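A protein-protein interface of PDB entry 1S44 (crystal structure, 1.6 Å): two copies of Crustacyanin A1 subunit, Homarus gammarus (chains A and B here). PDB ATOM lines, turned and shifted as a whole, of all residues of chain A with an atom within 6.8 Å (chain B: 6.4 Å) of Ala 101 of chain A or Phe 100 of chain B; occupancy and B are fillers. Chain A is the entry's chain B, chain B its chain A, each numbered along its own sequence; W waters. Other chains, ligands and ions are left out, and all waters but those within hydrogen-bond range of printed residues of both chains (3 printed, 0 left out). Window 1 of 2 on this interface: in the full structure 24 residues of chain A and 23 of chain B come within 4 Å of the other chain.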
ATOM      1  N   TYR A  83      18.011 -23.667   4.086  1.00  0.00           N
ATOM      2  CA  TYR A  83      18.911 -23.052   3.119  1.00  0.00           C
ATOM      3  C   TYR A  83      20.310 -22.980   3.652  1.00  0.00           C
ATOM      4  O   TYR A  83      20.561 -23.156   4.840  1.00  0.00           O
ATOM      5  CB  TYR A  83      18.410 -21.683   2.794  1.00  0.00           C
ATOM      6  CG  TYR A  83      17.996 -20.796   3.975  1.00  0.00           C
ATOM      7  CD1 TYR A  83      18.956 -20.128   4.717  1.00  0.00           C
ATOM      8  CD2 TYR A  83      16.675 -20.624   4.340  1.00  0.00           C
ATOM      9  CE1 TYR A  83      18.610 -19.319   5.765  1.00  0.00           C
ATOM     10  CE2 TYR A  83      16.312 -19.788   5.392  1.00  0.00           C
ATOM     11  CZ  TYR A  83      17.274 -19.136   6.089  1.00  0.00           C
ATOM     12  OH  TYR A  83      16.954 -18.309   7.166  1.00  0.00           O
ATOM     13  N   PHE A  87      26.561 -17.393   6.382  1.00  0.00           N
ATOM     14  CA  PHE A  87      27.991 -17.035   6.602  1.00  0.00           C
ATOM     15  C   PHE A  87      28.853 -17.943   5.735  1.00  0.00           C
ATOM     16  O   PHE A  87      30.088 -17.829   5.747  1.00  0.00           O
ATOM     17  CB  PHE A  87      28.396 -17.013   8.079  1.00  0.00           C
ATOM     18  CG  PHE A  87      27.674 -15.976   8.907  1.00  0.00           C
ATOM     19  CD1 PHE A  87      26.442 -16.257   9.483  1.00  0.00           C
ATOM     20  CD2 PHE A  87      28.192 -14.702   9.046  1.00  0.00           C
ATOM     21  CE1 PHE A  87      25.750 -15.353  10.248  1.00  0.00           C
ATOM     22  CE2 PHE A  87      27.487 -13.734   9.697  1.00  0.00           C
ATOM     23  CZ  PHE A  87      26.273 -14.041  10.334  1.00  0.00           C
ATOM     24  N   SER A  93      20.561 -23.878   7.435  1.00  0.00           N
ATOM     25  CA  SER A  93      19.745 -23.211   8.425  1.00  0.00           C
ATOM     26  C   SER A  93      18.343 -23.734   8.206  1.00  0.00           C
ATOM     27  O   SER A  93      17.855 -23.708   7.078  1.00  0.00           O
ATOM     28  CB  SER A  93      19.740 -21.714   8.162  1.00  0.00           C
ATOM     29  OG  SER A  93      20.993 -21.113   8.557  1.00  0.00           O
ATOM     30  N   ILE A  94      17.727 -24.255   9.261  1.00  0.00           N
ATOM     31  CA  ILE A  94      16.301 -24.559   9.231  1.00  0.00           C
ATOM     32  C   ILE A  94      15.561 -23.294   9.835  1.00  0.00           C
ATOM     33  O   ILE A  94      15.930 -22.833  10.885  1.00  0.00           O
ATOM     34  CB  ILE A  94      15.979 -25.850   9.985  1.00  0.00           C
ATOM     35  CG1 ILE A  94      14.477 -26.163   9.923  1.00  0.00           C
ATOM     36  CG2 ILE A  94      16.415 -25.783  11.382  1.00  0.00           C
ATOM     37  CD1 ILE A  94      14.006 -26.505   8.653  1.00  0.00           C
ATOM     38  N   ASP A  95      14.614 -22.759   9.094  1.00  0.00           N
ATOM     39  CA  ASP A  95      13.903 -21.487   9.407  1.00  0.00           C
ATOM     40  C   ASP A  95      12.425 -21.726   9.306  1.00  0.00           C
ATOM     41  O   ASP A  95      11.990 -22.388   8.442  1.00  0.00           O
ATOM     42  CB  ASP A  95      14.403 -20.416   8.474  1.00  0.00           C
ATOM     43  CG  ASP A  95      14.099 -19.007   8.926  1.00  0.00           C
ATOM     44  OD1 ASP A  95      14.640 -18.023   8.278  1.00  0.00           O
ATOM     45  OD2 ASP A  95      13.414 -18.857   9.970  1.00  0.00           O
ATOM     46  N   TYR A  96      11.643 -21.255  10.274  1.00  0.00           N
ATOM     47  CA  TYR A  96      10.203 -21.387  10.215  1.00  0.00           C
ATOM     48  C   TYR A  96       9.523 -20.029  10.430  1.00  0.00           C
ATOM     49  O   TYR A  96      10.039 -19.215  11.236  1.00  0.00           O
ATOM     50  CB  TYR A  96       9.697 -22.370  11.255  1.00  0.00           C
ATOM     51  CG  TYR A  96       9.730 -23.829  10.769  1.00  0.00           C
ATOM     52  CD1 TYR A  96      10.853 -24.578  10.885  1.00  0.00           C
ATOM     53  CD2 TYR A  96       8.646 -24.355  10.138  1.00  0.00           C
ATOM     54  CE1 TYR A  96      10.909 -25.938  10.379  1.00  0.00           C
ATOM     55  CE2 TYR A  96       8.664 -25.655   9.659  1.00  0.00           C
ATOM     56  CZ  TYR A  96       9.795 -26.424   9.784  1.00  0.00           C
ATOM     57  OH  TYR A  96       9.762 -27.719   9.341  1.00  0.00           O
ATOM     58  N   SER A  99       9.108 -17.922  13.951  1.00  0.00           N
ATOM     59  CA  SER A  99      10.064 -18.610  14.796  1.00  0.00           C
ATOM     60  C   SER A  99      11.493 -18.154  14.544  1.00  0.00           C
ATOM     61  O   SER A  99      11.762 -17.173  13.871  1.00  0.00           O
ATOM     62  CB  SER A  99       9.949 -20.110  14.555  1.00  0.00           C
ATOM     63  OG  SER A  99      10.719 -20.861  15.468  1.00  0.00           O
ATOM     64  N   PHE A 100      12.445 -18.902  14.992  1.00  0.00           N
ATOM     65  CA  PHE A 100      13.835 -18.535  14.736  1.00  0.00           C
ATOM     66  C   PHE A 100      14.371 -19.532  13.711  1.00  0.00           C
ATOM     67  O   PHE A 100      13.668 -20.418  13.264  1.00  0.00           O
ATOM     68  CB  PHE A 100      14.625 -18.660  15.963  1.00  0.00           C
ATOM     69  CG  PHE A 100      14.353 -19.878  16.648  1.00  0.00           C
ATOM     70  CD1 PHE A 100      15.177 -20.928  16.532  1.00  0.00           C
ATOM     71  CD2 PHE A 100      13.157 -20.033  17.362  1.00  0.00           C
ATOM     72  CE1 PHE A 100      14.852 -22.117  17.171  1.00  0.00           C
ATOM     73  CE2 PHE A 100      12.885 -21.180  18.002  1.00  0.00           C
ATOM     74  CZ  PHE A 100      13.706 -22.226  17.895  1.00  0.00           C
ATOM     75  N   ALA A 101      15.637 -19.359  13.360  1.00  0.00           N
ATOM     76  CA  ALA A 101      16.332 -20.263  12.523  1.00  0.00           C
ATOM     77  C   ALA A 101      17.491 -20.853  13.262  1.00  0.00           C
ATOM     78  O   ALA A 101      18.106 -20.227  14.049  1.00  0.00           O
ATOM     79  CB  ALA A 101      16.766 -19.540  11.207  1.00  0.00           C
ATOM     80  N   ALA A 102      17.824 -22.131  12.962  1.00  0.00           N
ATOM     81  CA  ALA A 102      18.863 -22.827  13.688  1.00  0.00           C
ATOM     82  C   ALA A 102      19.697 -23.697  12.740  1.00  0.00           C
ATOM     83  O   ALA A 102      19.253 -24.007  11.701  1.00  0.00           O
ATOM     84  CB  ALA A 102      18.295 -23.691  14.702  1.00  0.00           C
ATOM     85  N   PRO A 103      20.927 -23.992  13.094  1.00  0.00           N
ATOM     86  CA  PRO A 103      21.765 -24.869  12.273  1.00  0.00           C
ATOM     87  C   PRO A 103      21.152 -26.248  12.274  1.00  0.00           C
ATOM     88  O   PRO A 103      20.631 -26.741  13.260  1.00  0.00           O
ATOM     89  CB  PRO A 103      23.075 -24.909  13.036  1.00  0.00           C
ATOM     90  CG  PRO A 103      22.887 -24.195  14.230  1.00  0.00           C
ATOM     91  CD  PRO A 103      21.668 -23.485  14.269  1.00  0.00           C
ATOM     92  N   ILE A 121      23.610 -25.649  19.838  1.00  0.00           N
ATOM     93  CA  ILE A 121      23.921 -24.249  20.063  1.00  0.00           C
ATOM     94  C   ILE A 121      24.771 -24.204  21.360  1.00  0.00           C
ATOM     95  O   ILE A 121      24.451 -24.827  22.371  1.00  0.00           O
ATOM     96  CB  ILE A 121      22.682 -23.367  20.233  1.00  0.00           C
ATOM     97  CG1 ILE A 121      23.073 -21.855  20.408  1.00  0.00           C
ATOM     98  CG2 ILE A 121      21.858 -23.800  21.373  1.00  0.00           C
ATOM     99  CD1 ILE A 121      22.636 -20.956  19.258  1.00  0.00           C
ATOM    100  N   TYR B  44      23.100 -16.114  25.120  1.00  0.00           N
ATOM    101  CA  TYR B  44      23.712 -16.257  23.768  1.00  0.00           C
ATOM    102  C   TYR B  44      24.712 -15.168  23.464  1.00  0.00           C
ATOM    103  O   TYR B  44      25.370 -15.242  22.407  1.00  0.00           O
ATOM    104  CB  TYR B  44      22.676 -16.221  22.715  1.00  0.00           C
ATOM    105  CG  TYR B  44      21.535 -17.142  22.893  1.00  0.00           C
ATOM    106  CD1 TYR B  44      20.294 -16.686  23.228  1.00  0.00           C
ATOM    107  CD2 TYR B  44      21.668 -18.473  22.660  1.00  0.00           C
ATOM    108  CE1 TYR B  44      19.226 -17.507  23.387  1.00  0.00           C
ATOM    109  CE2 TYR B  44      20.565 -19.330  22.769  1.00  0.00           C
ATOM    110  CZ  TYR B  44      19.369 -18.858  23.187  1.00  0.00           C
ATOM    111  OH  TYR B  44      18.240 -19.682  23.328  1.00  0.00           O
ATOM    112  N   TYR B  83      19.084  -8.955   8.384  1.00  0.00           N
ATOM    113  CA  TYR B  83      18.422  -8.953   7.107  1.00  0.00           C
ATOM    114  C   TYR B  83      16.889  -9.221   7.267  1.00  0.00           C
ATOM    115  O   TYR B  83      16.416  -9.754   8.262  1.00  0.00           O
ATOM    116  CB  TYR B  83      19.025  -9.996   6.185  1.00  0.00           C
ATOM    117  CG  TYR B  83      19.259 -11.393   6.767  1.00  0.00           C
ATOM    118  CD1 TYR B  83      18.201 -12.296   6.871  1.00  0.00           C
ATOM    119  CD2 TYR B  83      20.488 -11.778   7.333  1.00  0.00           C
ATOM    120  CE1 TYR B  83      18.357 -13.537   7.404  1.00  0.00           C
ATOM    121  CE2 TYR B  83      20.670 -13.054   7.924  1.00  0.00           C
ATOM    122  CZ  TYR B  83      19.581 -13.930   7.907  1.00  0.00           C
ATOM    123  OH  TYR B  83      19.757 -15.190   8.413  1.00  0.00           O
ATOM    124  N   ILE B  94      18.242 -11.431  13.049  1.00  0.00           N
ATOM    125  CA  ILE B  94      19.604 -11.177  13.448  1.00  0.00           C
ATOM    126  C   ILE B  94      20.268 -12.529  13.516  1.00  0.00           C
ATOM    127  O   ILE B  94      19.784 -13.438  14.200  1.00  0.00           O
ATOM    128  CB  ILE B  94      19.666 -10.389  14.821  1.00  0.00           C
ATOM    129  CG1 ILE B  94      21.119 -10.128  15.264  1.00  0.00           C
ATOM    130  CG2 ILE B  94      19.036 -11.121  15.994  1.00  0.00           C
ATOM    131  CD1 ILE B  94      21.722  -8.826  14.878  1.00  0.00           C
ATOM    132  N   ASP B  95      21.391 -12.664  12.839  1.00  0.00           N
ATOM    133  CA  ASP B  95      22.021 -14.008  12.582  1.00  0.00           C
ATOM    134  C   ASP B  95      23.491 -13.876  12.843  1.00  0.00           C
ATOM    135  O   ASP B  95      24.146 -12.999  12.312  1.00  0.00           O
ATOM    136  CB  ASP B  95      21.827 -14.339  11.134  1.00  0.00           C
ATOM    137  CG  ASP B  95      22.167 -15.718  10.773  1.00  0.00           C
ATOM    138  OD1 ASP B  95      21.814 -16.111   9.640  1.00  0.00           O
ATOM    139  OD2 ASP B  95      22.733 -16.471  11.581  1.00  0.00           O
ATOM    140  N   TYR B  96      24.025 -14.684  13.708  1.00  0.00           N
ATOM    141  CA  TYR B  96      25.485 -14.621  13.984  1.00  0.00           C
ATOM    142  C   TYR B  96      26.125 -15.932  13.688  1.00  0.00           C
ATOM    143  O   TYR B  96      25.483 -16.960  13.884  1.00  0.00           O
ATOM    144  CB  TYR B  96      25.776 -14.278  15.415  1.00  0.00           C
ATOM    145  CG  TYR B  96      25.864 -12.842  15.714  1.00  0.00           C
ATOM    146  CD1 TYR B  96      24.734 -12.057  15.555  1.00  0.00           C
ATOM    147  CD2 TYR B  96      27.033 -12.201  15.996  1.00  0.00           C
ATOM    148  CE1 TYR B  96      24.758 -10.671  15.743  1.00  0.00           C
ATOM    149  CE2 TYR B  96      27.054 -10.833  16.189  1.00  0.00           C
ATOM    150  CZ  TYR B  96      25.912 -10.089  16.100  1.00  0.00           C
ATOM    151  OH  TYR B  96      25.990  -8.699  16.323  1.00  0.00           O
ATOM    152  N   GLU B  97      27.348 -15.870  13.149  1.00  0.00           N
ATOM    153  CA  GLU B  97      28.191 -17.039  12.863  1.00  0.00           C
ATOM    154  C   GLU B  97      28.334 -17.923  14.069  1.00  0.00           C
ATOM    155  O   GLU B  97      28.502 -17.475  15.211  1.00  0.00           O
ATOM    156  CB  GLU B  97      29.589 -16.584  12.460  1.00  0.00           C
ATOM    157  CG  GLU B  97      30.452 -17.589  11.707  1.00  0.00           C
ATOM    158  CD  GLU B  97      31.716 -16.884  11.191  1.00  0.00           C
ATOM    159  OE1 GLU B  97      32.347 -16.147  11.977  1.00  0.00           O
ATOM    160  OE2 GLU B  97      32.034 -17.013   9.991  1.00  0.00           O
ATOM    161  N   ASN B  98      28.250 -19.224  13.834  1.00  0.00           N
ATOM    162  CA  ASN B  98      28.374 -20.197  14.906  1.00  0.00           C
ATOM    163  C   ASN B  98      27.269 -20.011  15.955  1.00  0.00           C
ATOM    164  O   ASN B  98      27.439 -20.319  17.106  1.00  0.00           O
ATOM    165  CB  ASN B  98      29.801 -20.266  15.533  1.00  0.00           C
ATOM    166  CG  ASN B  98      30.907 -20.414  14.493  1.00  0.00           C
ATOM    167  OD1 ASN B  98      31.858 -19.636  14.479  1.00  0.00           O
ATOM    168  ND2 ASN B  98      30.789 -21.405  13.625  1.00  0.00           N
ATOM    169  N   SER B  99      26.078 -19.585  15.536  1.00  0.00           N
ATOM    170  CA  SER B  99      24.983 -19.387  16.463  1.00  0.00           C
ATOM    171  C   SER B  99      23.699 -19.607  15.697  1.00  0.00           C
ATOM    172  O   SER B  99      23.679 -20.170  14.651  1.00  0.00           O
ATOM    173  CB  SER B  99      25.021 -17.976  17.008  1.00  0.00           C
ATOM    174  OG  SER B  99      24.237 -17.772  18.142  1.00  0.00           O
ATOM    175  N   PHE B 100      22.647 -19.043  16.156  1.00  0.00           N
ATOM    176  CA  PHE B 100      21.387 -19.166  15.449  1.00  0.00           C
ATOM    177  C   PHE B 100      20.888 -17.807  15.013  1.00  0.00           C
ATOM    178  O   PHE B 100      21.619 -16.812  15.157  1.00  0.00           O
ATOM    179  CB  PHE B 100      20.449 -19.888  16.293  1.00  0.00           C
ATOM    180  CG  PHE B 100      19.760 -19.085  17.298  1.00  0.00           C
ATOM    181  CD1 PHE B 100      20.380 -18.693  18.449  1.00  0.00           C
ATOM    182  CD2 PHE B 100      18.444 -18.832  17.124  1.00  0.00           C
ATOM    183  CE1 PHE B 100      19.656 -17.975  19.397  1.00  0.00           C
ATOM    184  CE2 PHE B 100      17.731 -18.182  18.016  1.00  0.00           C
ATOM    185  CZ  PHE B 100      18.353 -17.722  19.169  1.00  0.00           C
ATOM    186  N   ALA B 101      19.738 -17.759  14.334  1.00  0.00           N
ATOM    187  CA  ALA B 101      19.174 -16.486  13.904  1.00  0.00           C
ATOM    188  C   ALA B 101      17.839 -16.303  14.588  1.00  0.00           C
ATOM    189  O   ALA B 101      17.107 -17.263  14.752  1.00  0.00           O
ATOM    190  CB  ALA B 101      19.004 -16.483  12.463  1.00  0.00           C
ATOM    191  N   ALA B 102      17.509 -15.081  14.995  1.00  0.00           N
ATOM    192  CA  ALA B 102      16.281 -14.794  15.749  1.00  0.00           C
ATOM    193  C   ALA B 102      15.609 -13.538  15.210  1.00  0.00           C
ATOM    194  O   ALA B 102      16.261 -12.707  14.614  1.00  0.00           O
ATOM    195  CB  ALA B 102      16.655 -14.481  17.140  1.00  0.00           C
ATOM    196  N   PRO B 103      14.320 -13.367  15.434  1.00  0.00           N
ATOM    197  CA  PRO B 103      13.688 -12.120  15.085  1.00  0.00           C
ATOM    198  C   PRO B 103      14.241 -10.974  15.929  1.00  0.00           C
ATOM    199  O   PRO B 103      14.583 -11.131  17.112  1.00  0.00           O
ATOM    200  CB  PRO B 103      12.217 -12.335  15.448  1.00  0.00           C
ATOM    201  CG  PRO B 103      12.260 -13.433  16.431  1.00  0.00           C
ATOM    202  CD  PRO B 103      13.399 -14.261  16.159  1.00  0.00           C
ATOM    203  N   SER B 119      13.680  -9.197  20.916  1.00  0.00           N
ATOM    204  CA  SER B 119      13.569 -10.511  20.232  1.00  0.00           C
ATOM    205  C   SER B 119      12.712 -11.378  21.126  1.00  0.00           C
ATOM    206  O   SER B 119      12.864 -11.404  22.334  1.00  0.00           O
ATOM    207  CB  SER B 119      14.958 -11.123  20.066  1.00  0.00           C
ATOM    208  OG  SER B 119      14.932 -12.400  19.433  1.00  0.00           O
ATOM    209  N   ILE B 121      10.873 -15.548  21.412  1.00  0.00           N
ATOM    210  CA  ILE B 121      10.676 -16.892  20.850  1.00  0.00           C
ATOM    211  C   ILE B 121       9.606 -17.550  21.770  1.00  0.00           C
ATOM    212  O   ILE B 121       9.660 -17.464  22.993  1.00  0.00           O
ATOM    213  CB  ILE B 121      11.942 -17.699  20.902  1.00  0.00           C
ATOM    214  CG1 ILE B 121      13.090 -17.004  20.172  1.00  0.00           C
ATOM    215  CG2 ILE B 121      11.706 -19.161  20.410  1.00  0.00           C
ATOM    216  CD1 ILE B 121      13.752 -16.064  21.196  1.00  0.00           C
ATOM    217  N   PHE B 131      14.453 -11.317  24.789  1.00  0.00           N
ATOM    218  CA  PHE B 131      15.766 -10.785  24.951  1.00  0.00           C
ATOM    219  C   PHE B 131      15.743  -9.359  24.416  1.00  0.00           C
ATOM    220  O   PHE B 131      15.299  -9.100  23.288  1.00  0.00           O
ATOM    221  CB  PHE B 131      16.732 -11.672  24.155  1.00  0.00           C
ATOM    222  CG  PHE B 131      16.644 -13.123  24.585  1.00  0.00           C
ATOM    223  CD1 PHE B 131      15.898 -14.011  23.866  1.00  0.00           C
ATOM    224  CD2 PHE B 131      17.230 -13.528  25.749  1.00  0.00           C
ATOM    225  CE1 PHE B 131      15.818 -15.312  24.235  1.00  0.00           C
ATOM    226  CE2 PHE B 131      17.149 -14.836  26.173  1.00  0.00           C
ATOM    227  CZ  PHE B 131      16.450 -15.701  25.440  1.00  0.00           C
HETATM  228  O   HOH W   1      20.574 -18.665   9.803  1.00  0.00           O
HETATM  229  O   HOH W   2      18.240 -17.183   9.172  1.00  0.00           O
HETATM  230  O   HOH W   3      31.920 -19.187   8.015  1.00  0.00           O
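The backbone carbonyl oxygen (O) of Ala 101 of chain B is in hydrogen-bond range of the backbone NH (N) of Ala 101 of chain A (2.9 Å).
The side-chain carboxylate (OD1) of Asp 95 of chain B sits at hydrogen-bond distance from the side-chain hydroxyl (OH) of Tyr 83 of chain B (2.6 Å).
Among the printed residues, pairs that only touch across the chains: Phe 87 of chain A with Asp 95 of chain B (3.1 Å), Phe 100 of chain A with Ala 101 of chain B (3.1 Å), Ala 101 of chain A with Phe 100 of chain B (3.3 Å), Ile 121 of chain A with Phe 100 of chain B (3.3 Å), Phe 87 of chain A with Glu 97 of chain B (3.4 Å), Phe 100 of chain A with Ile 121 of chain B (3.4 Å), Phe 87 of chain A with Tyr 96 of chain B (3.5 Å), Ile 121 of chain A with Ser 99 of chain B (3.7 Å), Phe 100 of chain A with Phe 100 of chain B (3.8 Å) and Pro 103 of chain A with Ser 99 of chain B (3.9 Å).
Printed residues of chain A within 4 Å of Ala 101 of chain B: Phe 100 (3.1 Å) and Ala 101 (2.9 Å). Of the printed residues of chain B, Phe 87 of chain A touches Asp 95 (3.1 Å), Tyr 96 (3.5 Å) and Glu 97 (3.4 Å). Printed residues of chain A within 4 Å of Asp 95 of chain B: Phe 87 (3.1 Å). Of the printed residues of chain A, Ser 99 of chain B touches Pro 103 and Ile 121. Printed residues of chain B within 4 Å of Ile 121 of chain A: Ser 99 and Phe 100. Ser 93 of chain A touches none of the printed residues of chain B. The nearest printed residue of chain A that does not touch Ser 99 of chain B is Ala 102 of chain A (5.6 Å).
Of the 15 printed residues of chain B, 7 touch a printed residue of chain A. Hydrophobic or aromatic side chains of chain B within 4 Å of the printed part of chain A: Phe 100, Ala 101 and Ile 121. Of the 12 printed residues of chain A, 5 touch a printed residue of chain B. Among the printed residues, 11 pairs touch across the chains.
Phe 100 of chain A touches its own counterpart, Phe 100 of chain B. Phe 100 of chain A touches Ile 121 of chain B, and with the chains exchanged Ile 121 of chain A touches Phe 100 of chain B. Ala 101 of chain A touches its own counterpart, Ala 101 of chain B. Pro 103 of chain A touches Ser 99 of chain B, but with the chains exchanged Ser 99 of chain A does not touch Pro 103 of chain B (4.05 Å). Positions printed for both chains: 83, 94, 95, 96, 99, 100, 101, 102, 103 and 121. Of the 11 pairs that touch across the chains among the printed residues, 6 have their exchanged pair printed and touching as well.
Water W2 bridges the side-chain hydroxyl of Tyr 83 of chain B (2.6 Å) and the side-chain hydroxyl of Tyr 83 of chain A (2.6 Å). Water W1 lies within hydrogen-bond range of OG of Ser 93 of chain A (2.8 Å) and OD1 of Asp 95 of chain B (2.8 Å). Water W3 lies within hydrogen-bond range of the side-chain carboxylate (OE2) of Glu 97 of chain B (2.9 Å) and the backbone carbonyl oxygen (O) of Phe 87 of chain A (3.2 Å).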
